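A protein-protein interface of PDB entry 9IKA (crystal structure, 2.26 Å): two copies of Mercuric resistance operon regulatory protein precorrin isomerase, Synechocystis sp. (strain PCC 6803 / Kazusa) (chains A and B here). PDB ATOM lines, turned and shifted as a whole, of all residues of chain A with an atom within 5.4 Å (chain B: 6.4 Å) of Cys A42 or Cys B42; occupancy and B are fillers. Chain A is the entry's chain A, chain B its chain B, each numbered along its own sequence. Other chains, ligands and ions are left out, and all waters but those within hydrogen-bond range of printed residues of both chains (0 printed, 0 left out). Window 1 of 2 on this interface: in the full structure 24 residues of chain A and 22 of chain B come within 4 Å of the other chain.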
ATOM      1  N   LEU A  38      12.483  14.831 -29.313  1.00  0.00           N
ATOM      2  CA  LEU A  38      11.860  14.790 -28.001  1.00  0.00           C
ATOM      3  C   LEU A  38      12.020  13.396 -27.390  1.00  0.00           C
ATOM      4  O   LEU A  38      12.309  13.273 -26.199  1.00  0.00           O
ATOM      5  CB  LEU A  38      10.398  15.227 -28.077  1.00  0.00           C
ATOM      6  CG  LEU A  38      10.158  16.729 -28.276  1.00  0.00           C
ATOM      7  CD1 LEU A  38       8.678  17.028 -28.415  1.00  0.00           C
ATOM      8  CD2 LEU A  38      10.745  17.564 -27.155  1.00  0.00           C
ATOM      9  N   VAL A  39      11.847  12.356 -28.212  1.00  0.00           N
ATOM     10  CA  VAL A  39      12.056  10.983 -27.775  1.00  0.00           C
ATOM     11  C   VAL A  39      13.513  10.779 -27.361  1.00  0.00           C
ATOM     12  O   VAL A  39      13.763  10.153 -26.337  1.00  0.00           O
ATOM     13  CB  VAL A  39      11.625   9.972 -28.853  1.00  0.00           C
ATOM     14  CG1 VAL A  39      12.193   8.579 -28.605  1.00  0.00           C
ATOM     15  CG2 VAL A  39      10.108   9.917 -28.977  1.00  0.00           C
ATOM     16  N   LEU A  40      14.459  11.320 -28.146  1.00  0.00           N
ATOM     17  CA  LEU A  40      15.879  11.189 -27.857  1.00  0.00           C
ATOM     18  C   LEU A  40      16.231  11.878 -26.539  1.00  0.00           C
ATOM     19  O   LEU A  40      17.221  11.517 -25.918  1.00  0.00           O
ATOM     20  CB  LEU A  40      16.755  11.747 -28.980  1.00  0.00           C
ATOM     21  CG  LEU A  40      16.890  10.900 -30.250  1.00  0.00           C
ATOM     22  CD1 LEU A  40      17.861  11.601 -31.191  1.00  0.00           C
ATOM     23  CD2 LEU A  40      17.347   9.474 -29.997  1.00  0.00           C
ATOM     24  N   ALA A  41      15.446  12.883 -26.138  1.00  0.00           N
ATOM     25  CA  ALA A  41      15.754  13.682 -24.963  1.00  0.00           C
ATOM     26  C   ALA A  41      15.516  12.879 -23.687  1.00  0.00           C
ATOM     27  O   ALA A  41      16.345  12.911 -22.783  1.00  0.00           O
ATOM     28  CB  ALA A  41      14.941  14.957 -24.963  1.00  0.00           C
ATOM     29  N   CYS A  42      14.383  12.169 -23.620  1.00  0.00           N
ATOM     30  CA  CYS A  42      13.920  11.601 -22.362  1.00  0.00           C
ATOM     31  C   CYS A  42      13.579  10.117 -22.479  1.00  0.00           C
ATOM     32  O   CYS A  42      13.333   9.486 -21.457  1.00  0.00           O
ATOM     33  CB  CYS A  42      12.700  12.356 -21.858  1.00  0.00           C
ATOM     34  SG  CYS A  42      11.255  12.147 -22.930  1.00  0.00           S
ATOM     35  N   GLY A  43      13.518   9.576 -23.704  1.00  0.00           N
ATOM     36  CA  GLY A  43      13.378   8.144 -23.926  1.00  0.00           C
ATOM     37  C   GLY A  43      11.928   7.656 -24.022  1.00  0.00           C
ATOM     38  O   GLY A  43      11.701   6.462 -24.208  1.00  0.00           O
ATOM     39  N   ASP A  44      10.941   8.553 -23.911  1.00  0.00           N
ATOM     40  CA  ASP A  44       9.551   8.130 -23.812  1.00  0.00           C
ATOM     41  C   ASP A  44       8.886   8.163 -25.185  1.00  0.00           C
ATOM     42  O   ASP A  44       8.556   9.231 -25.691  1.00  0.00           O
ATOM     43  CB  ASP A  44       8.788   8.953 -22.785  1.00  0.00           C
ATOM     44  CG  ASP A  44       7.416   8.410 -22.402  1.00  0.00           C
ATOM     45  OD1 ASP A  44       6.816   7.664 -23.216  1.00  0.00           O
ATOM     46  OD2 ASP A  44       6.974   8.695 -21.269  1.00  0.00           O
ATOM     47  N   LEU A  47       5.582   9.997 -26.327  1.00  0.00           N
ATOM     48  CA  LEU A  47       5.597  11.419 -26.638  1.00  0.00           C
ATOM     49  C   LEU A  47       5.040  11.690 -28.034  1.00  0.00           C
ATOM     50  O   LEU A  47       4.467  12.756 -28.254  1.00  0.00           O
ATOM     51  CB  LEU A  47       6.994  12.031 -26.512  1.00  0.00           C
ATOM     52  CG  LEU A  47       7.335  12.661 -25.160  1.00  0.00           C
ATOM     53  CD1 LEU A  47       8.801  13.035 -25.118  1.00  0.00           C
ATOM     54  CD2 LEU A  47       6.470  13.882 -24.888  1.00  0.00           C
ATOM     55  N   ILE A 163       5.924  21.475 -15.709  1.00  0.00           N
ATOM     56  CA  ILE A 163       5.940  20.279 -14.876  1.00  0.00           C
ATOM     57  C   ILE A 163       4.514  19.982 -14.409  1.00  0.00           C
ATOM     58  O   ILE A 163       3.683  20.884 -14.354  1.00  0.00           O
ATOM     59  CB  ILE A 163       6.922  20.486 -13.700  1.00  0.00           C
ATOM     60  CG1 ILE A 163       8.358  20.670 -14.187  1.00  0.00           C
ATOM     61  CG2 ILE A 163       6.841  19.361 -12.669  1.00  0.00           C
ATOM     62  CD1 ILE A 163       8.857  19.550 -15.082  1.00  0.00           C
ATOM     63  N   LEU A 189       3.910  14.781 -18.883  1.00  0.00           N
ATOM     64  CA  LEU A 189       5.279  15.076 -19.283  1.00  0.00           C
ATOM     65  C   LEU A 189       5.441  16.560 -19.617  1.00  0.00           C
ATOM     66  O   LEU A 189       4.478  17.237 -19.972  1.00  0.00           O
ATOM     67  CB  LEU A 189       5.708  14.205 -20.463  1.00  0.00           C
ATOM     68  CG  LEU A 189       6.017  12.738 -20.145  1.00  0.00           C
ATOM     69  CD1 LEU A 189       4.753  11.930 -19.875  1.00  0.00           C
ATOM     70  CD2 LEU A 189       6.822  12.116 -21.276  1.00  0.00           C
ATOM     71  N   GLY A 190       6.690  17.030 -19.522  1.00  0.00           N
ATOM     72  CA  GLY A 190       7.060  18.419 -19.740  1.00  0.00           C
ATOM     73  C   GLY A 190       8.476  18.661 -19.224  1.00  0.00           C
ATOM     74  O   GLY A 190       9.219  17.712 -19.014  1.00  0.00           O
ATOM     75  N   GLY A 191       8.864  19.924 -19.036  1.00  0.00           N
ATOM     76  CA  GLY A 191      10.087  20.223 -18.313  1.00  0.00           C
ATOM     77  C   GLY A 191      11.021  21.140 -19.092  1.00  0.00           C
ATOM     78  O   GLY A 191      10.722  21.557 -20.207  1.00  0.00           O
ATOM     79  N   GLY A 192      12.163  21.436 -18.469  1.00  0.00           N
ATOM     80  CA  GLY A 192      13.094  22.426 -18.979  1.00  0.00           C
ATOM     81  C   GLY A 192      13.776  21.940 -20.254  1.00  0.00           C
ATOM     82  O   GLY A 192      13.859  22.674 -21.242  1.00  0.00           O
ATOM     83  N   LEU A 193      14.252  20.693 -20.224  1.00  0.00           N
ATOM     84  CA  LEU A 193      14.889  20.110 -21.388  1.00  0.00           C
ATOM     85  C   LEU A 193      13.883  20.059 -22.542  1.00  0.00           C
ATOM     86  O   LEU A 193      14.238  20.412 -23.664  1.00  0.00           O
ATOM     87  CB  LEU A 193      15.463  18.735 -21.030  1.00  0.00           C
ATOM     88  CG  LEU A 193      16.355  18.059 -22.081  1.00  0.00           C
ATOM     89  CD1 LEU A 193      17.549  18.932 -22.454  1.00  0.00           C
ATOM     90  CD2 LEU A 193      16.839  16.697 -21.601  1.00  0.00           C
ATOM     91  N   LEU A 194      12.630  19.661 -22.276  1.00  0.00           N
ATOM     92  CA  LEU A 194      11.690  19.392 -23.358  1.00  0.00           C
ATOM     93  C   LEU A 194      11.295  20.691 -24.058  1.00  0.00           C
ATOM     94  O   LEU A 194      11.137  20.696 -25.277  1.00  0.00           O
ATOM     95  CB  LEU A 194      10.444  18.624 -22.917  1.00  0.00           C
ATOM     96  CG  LEU A 194      10.664  17.208 -22.365  1.00  0.00           C
ATOM     97  CD1 LEU A 194       9.341  16.456 -22.364  1.00  0.00           C
ATOM     98  CD2 LEU A 194      11.720  16.401 -23.105  1.00  0.00           C
ATOM     99  N   GLN B  37      17.101  17.288 -10.698  1.00  0.00           N
ATOM    100  CA  GLN B  37      17.496  17.730 -12.029  1.00  0.00           C
ATOM    101  C   GLN B  37      16.841  16.874 -13.114  1.00  0.00           C
ATOM    102  O   GLN B  37      16.444  17.404 -14.146  1.00  0.00           O
ATOM    103  CB  GLN B  37      19.017  17.715 -12.188  1.00  0.00           C
ATOM    104  CG  GLN B  37      19.759  18.696 -11.285  1.00  0.00           C
ATOM    105  CD  GLN B  37      19.388  20.141 -11.536  1.00  0.00           C
ATOM    106  OE1 GLN B  37      18.400  20.653 -11.004  1.00  0.00           O
ATOM    107  NE2 GLN B  37      20.192  20.823 -12.339  1.00  0.00           N
ATOM    108  N   LEU B  38      16.729  15.560 -12.868  1.00  0.00           N
ATOM    109  CA  LEU B  38      16.158  14.622 -13.824  1.00  0.00           C
ATOM    110  C   LEU B  38      14.650  14.828 -13.980  1.00  0.00           C
ATOM    111  O   LEU B  38      14.136  14.739 -15.095  1.00  0.00           O
ATOM    112  CB  LEU B  38      16.482  13.196 -13.380  1.00  0.00           C
ATOM    113  CG  LEU B  38      17.964  12.811 -13.392  1.00  0.00           C
ATOM    114  CD1 LEU B  38      18.184  11.467 -12.721  1.00  0.00           C
ATOM    115  CD2 LEU B  38      18.493  12.790 -14.809  1.00  0.00           C
ATOM    116  N   VAL B  39      13.951  15.082 -12.864  1.00  0.00           N
ATOM    117  CA  VAL B  39      12.529  15.397 -12.887  1.00  0.00           C
ATOM    118  C   VAL B  39      12.290  16.751 -13.563  1.00  0.00           C
ATOM    119  O   VAL B  39      11.338  16.896 -14.333  1.00  0.00           O
ATOM    120  CB  VAL B  39      11.933  15.359 -11.467  1.00  0.00           C
ATOM    121  CG1 VAL B  39      10.503  15.884 -11.425  1.00  0.00           C
ATOM    122  CG2 VAL B  39      11.992  13.955 -10.878  1.00  0.00           C
ATOM    123  N   LEU B  40      13.145  17.742 -13.269  1.00  0.00           N
ATOM    124  CA  LEU B  40      13.025  19.064 -13.874  1.00  0.00           C
ATOM    125  C   LEU B  40      13.226  18.983 -15.388  1.00  0.00           C
ATOM    126  O   LEU B  40      12.681  19.808 -16.117  1.00  0.00           O
ATOM    127  CB  LEU B  40      14.005  20.068 -13.265  1.00  0.00           C
ATOM    128  CG  LEU B  40      13.591  20.709 -11.936  1.00  0.00           C
ATOM    129  CD1 LEU B  40      14.762  21.457 -11.302  1.00  0.00           C
ATOM    130  CD2 LEU B  40      12.420  21.651 -12.119  1.00  0.00           C
ATOM    131  N   ALA B  41      14.020  18.007 -15.852  1.00  0.00           N
ATOM    132  CA  ALA B  41      14.341  17.888 -17.266  1.00  0.00           C
ATOM    133  C   ALA B  41      13.150  17.359 -18.071  1.00  0.00           C
ATOM    134  O   ALA B  41      12.825  17.933 -19.108  1.00  0.00           O
ATOM    135  CB  ALA B  41      15.566  17.023 -17.458  1.00  0.00           C
ATOM    136  N   CYS B  42      12.506  16.278 -17.603  1.00  0.00           N
ATOM    137  CA  CYS B  42      11.527  15.566 -18.419  1.00  0.00           C
ATOM    138  C   CYS B  42      10.163  15.405 -17.743  1.00  0.00           C
ATOM    139  O   CYS B  42       9.233  14.923 -18.386  1.00  0.00           O
ATOM    140  CB  CYS B  42      12.033  14.179 -18.799  1.00  0.00           C
ATOM    141  SG  CYS B  42      12.104  13.034 -17.395  1.00  0.00           S
ATOM    142  N   GLY B  43      10.038  15.760 -16.458  1.00  0.00           N
ATOM    143  CA  GLY B  43       8.738  15.817 -15.804  1.00  0.00           C
ATOM    144  C   GLY B  43       8.274  14.491 -15.189  1.00  0.00           C
ATOM    145  O   GLY B  43       7.225  14.457 -14.546  1.00  0.00           O
ATOM    146  N   ASP B  44       9.042  13.401 -15.346  1.00  0.00           N
ATOM    147  CA  ASP B  44       8.597  12.104 -14.857  1.00  0.00           C
ATOM    148  C   ASP B  44       8.977  11.914 -13.387  1.00  0.00           C
ATOM    149  O   ASP B  44      10.141  11.668 -13.069  1.00  0.00           O
ATOM    150  CB  ASP B  44       9.128  10.963 -15.710  1.00  0.00           C
ATOM    151  CG  ASP B  44       8.554   9.593 -15.368  1.00  0.00           C
ATOM    152  OD1 ASP B  44       7.618   9.530 -14.535  1.00  0.00           O
ATOM    153  OD2 ASP B  44       9.053   8.595 -15.925  1.00  0.00           O
ATOM    154  N   LEU B  47      10.942   8.750 -11.699  1.00  0.00           N
ATOM    155  CA  LEU B  47      12.391   8.608 -11.753  1.00  0.00           C
ATOM    156  C   LEU B  47      13.005   8.511 -10.352  1.00  0.00           C
ATOM    157  O   LEU B  47      14.102   7.975 -10.195  1.00  0.00           O
ATOM    158  CB  LEU B  47      13.000   9.762 -12.552  1.00  0.00           C
ATOM    159  CG  LEU B  47      12.859   9.680 -14.077  1.00  0.00           C
ATOM    160  CD1 LEU B  47      13.337  10.968 -14.708  1.00  0.00           C
ATOM    161  CD2 LEU B  47      13.622   8.520 -14.681  1.00  0.00           C
ATOM    162  N   ILE B 163      18.353   4.265 -25.050  1.00  0.00           N
ATOM    163  CA  ILE B 163      16.986   4.283 -25.543  1.00  0.00           C
ATOM    164  C   ILE B 163      16.482   2.844 -25.569  1.00  0.00           C
ATOM    165  O   ILE B 163      17.277   1.918 -25.722  1.00  0.00           O
ATOM    166  CB  ILE B 163      16.947   4.958 -26.929  1.00  0.00           C
ATOM    167  CG1 ILE B 163      17.312   6.446 -26.848  1.00  0.00           C
ATOM    168  CG2 ILE B 163      15.607   4.760 -27.635  1.00  0.00           C
ATOM    169  CD1 ILE B 163      16.319   7.301 -26.080  1.00  0.00           C
ATOM    170  N   LEU B 189      10.945   4.669 -18.443  1.00  0.00           N
ATOM    171  CA  LEU B 189      11.332   4.664 -19.848  1.00  0.00           C
ATOM    172  C   LEU B 189      12.497   5.627 -20.077  1.00  0.00           C
ATOM    173  O   LEU B 189      12.975   5.760 -21.203  1.00  0.00           O
ATOM    174  CB  LEU B 189      10.134   5.010 -20.735  1.00  0.00           C
ATOM    175  CG  LEU B 189       9.072   3.916 -20.903  1.00  0.00           C
ATOM    176  CD1 LEU B 189       7.913   4.436 -21.740  1.00  0.00           C
ATOM    177  CD2 LEU B 189       9.654   2.646 -21.520  1.00  0.00           C
ATOM    178  N   GLY B 190      12.957   6.279 -19.003  1.00  0.00           N
ATOM    179  CA  GLY B 190      14.069   7.213 -19.070  1.00  0.00           C
ATOM    180  C   GLY B 190      15.231   6.684 -19.911  1.00  0.00           C
ATOM    181  O   GLY B 190      15.616   5.525 -19.795  1.00  0.00           O
ATOM    182  N   GLY B 191      15.773   7.565 -20.757  1.00  0.00           N
ATOM    183  CA  GLY B 191      16.995   7.317 -21.504  1.00  0.00           C
ATOM    184  C   GLY B 191      17.395   8.576 -22.263  1.00  0.00           C
ATOM    185  O   GLY B 191      16.814   9.633 -22.040  1.00  0.00           O
ATOM    186  N   GLY B 192      18.384   8.462 -23.154  1.00  0.00           N
ATOM    187  CA  GLY B 192      18.762   9.567 -24.016  1.00  0.00           C
ATOM    188  C   GLY B 192      19.586  10.613 -23.270  1.00  0.00           C
ATOM    189  O   GLY B 192      20.512  10.264 -22.540  1.00  0.00           O
ATOM    190  N   LEU B 193      19.193  11.889 -23.434  1.00  0.00           N
ATOM    191  CA  LEU B 193      19.912  13.040 -22.899  1.00  0.00           C
ATOM    192  C   LEU B 193      19.809  13.124 -21.374  1.00  0.00           C
ATOM    193  O   LEU B 193      20.466  13.963 -20.764  1.00  0.00           O
ATOM    194  CB  LEU B 193      19.381  14.321 -23.546  1.00  0.00           C
ATOM    195  CG  LEU B 193      19.517  14.427 -25.070  1.00  0.00           C
ATOM    196  CD1 LEU B 193      19.083  15.805 -25.556  1.00  0.00           C
ATOM    197  CD2 LEU B 193      20.933  14.129 -25.545  1.00  0.00           C
ATOM    198  N   LEU B 194      19.005  12.255 -20.750  1.00  0.00           N
ATOM    199  CA  LEU B 194      19.076  12.074 -19.308  1.00  0.00           C
ATOM    200  C   LEU B 194      20.479  11.633 -18.889  1.00  0.00           C
ATOM    201  O   LEU B 194      20.891  11.895 -17.767  1.00  0.00           O
ATOM    202  CB  LEU B 194      18.004  11.093 -18.840  1.00  0.00           C
ATOM    203  CG  LEU B 194      16.552  11.526 -19.079  1.00  0.00           C
ATOM    204  CD1 LEU B 194      15.602  10.531 -18.445  1.00  0.00           C
ATOM    205  CD2 LEU B 194      16.257  12.925 -18.561  1.00  0.00           C
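Val A39 touches Ile B163, and with the chains exchanged Ile A163 touches Val B39.
Leu A40 touches Gly B192, and with the chains exchanged Gly A192 touches Leu B40.
Gly A43 touches Gly B191, but with the chains exchanged Gly A191 does not touch Gly B43 (4.8 Å).
Gly A191 touches Leu B40, but with the chains exchanged Leu A40 does not touch Gly B191 (4.3 Å).
15 positions are printed for both chains.
Of the 28 pairs that touch across the chains among the printed residues, 16 have their exchanged pair printed and touching as well.
Among the printed residues, merely in contact across the chains: Leu A40 with Gly B192 (3.1 Å), Cys A42 with Gly B190 (3.4 Å), Gly A191 with Leu B40 (3.4 Å), Leu A194 with Ala B41 (3.6 Å), Gly A190 with Ala B41 (3.6 Å), Gly A192 with Ala B41 (3.6 Å), Cys A42 with Cys B42 (3.6 Å), Gly A191 with Ala B41 (3.7 Å), Gly A43 with Gly B191 (3.7 Å), Ile A163 with Val B39 (3.7 Å), Asp A44 with Leu B189 (3.7 Å), Gly A43 with Ile B163 (3.7 Å), Cys A42 with Leu B189 (3.8 Å), Ile A163 with Gly B43 (3.8 Å), Val A39 with Ile B163 (3.8 Å), Cys A42 with Leu B194 (3.9 Å), Ile A163 with Leu B40 (3.97 Å) and Leu A193 with Leu B193 (3.99 Å).
Along chain B the printed residues that touch a printed residue of chain A span positions 39 to 194.
Hydrophobic or aromatic side chains of chain A within 4 Å of the printed part of chain B: Ile A163, Leu A193 and Leu A194.
Along chain A the printed residues that touch a printed residue of chain B span positions 39 to 194.
Among the printed residues, no Asp or Glu carboxylate lies within 4 Å of a Lys or Arg side-chain nitrogen of the other chain.
SG of Cys B42 sits close to N of Asp B44, 3.7 Å away.
The side-chain sulfur (SG) of Cys B42 sits at hydrogen-bond distance from the backbone carbonyl oxygen (O) of Leu B38 (3.5 Å).
The side-chain sulfur (SG) of Cys A42 lies close to the backbone NH (N) of Asp A44, at 3.7 Å.
O of Leu A38 lies within hydrogen-bond range of SG of Cys A42 (3.6 Å).
N of Leu B193 is in hydrogen-bond range of O of Leu A40 (3.2 Å).
The backbone NH (N) of Leu A193 sits at hydrogen-bond distance from the backbone carbonyl oxygen (O) of Ala B41 (3.3 Å).
O of Gly A43 lies close to O of Leu B189.
The backbone NH (N) of Leu B194 sits at hydrogen-bond distance from the backbone carbonyl oxygen (O) of Ala A41, at 3.4 Å.
O of Ala A41 is in hydrogen-bond range of N of Leu B193.
O of Gly A190 is in hydrogen-bond range of N of Gly B43 (3.3 Å).
The backbone carbonyl oxygen (O) of Cys A42 is in hydrogen-bond range of the backbone NH (N) of Gly B191 (3.2 Å).
The backbone carbonyl oxygen of Cys B42 lies within hydrogen-bond range of the backbone NH of Gly A190, 3.5 Å away.
The backbone carbonyl oxygen of Ala A41 lies close to the backbone carbonyl oxygen of Gly B191 (3.4 Å).
The backbone carbonyl oxygen (O) of Leu B40 sits at hydrogen-bond distance from the backbone NH (N) of Gly A192, at 2.9 Å.
Of the printed residues of chain B, Ala A41 touches Gly B191 (3.4 Å), Leu B193 (3.1 Å) and Leu B194 (3.4 Å).
Cys A42 touches just these residues of chain B: Cys B42 (3.6 Å), Leu B189 (3.8 Å), Gly B190 (3.4 Å), Gly B191 (3.2 Å) and Leu B194 (3.9 Å).
Of the printed residues of chain A, Cys B42 touches Cys A42 and Gly A190.
Of the printed residues of chain A, Gly B191 touches Ala A41 (3.4 Å), Cys A42 (3.2 Å) and Gly A43 (3.7 Å).
Of the printed residues of chain A, Gly B192 touches Leu A40.
The nearest residue of chain B that does not touch Cys A42 is Leu B193 (4.8 Å).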
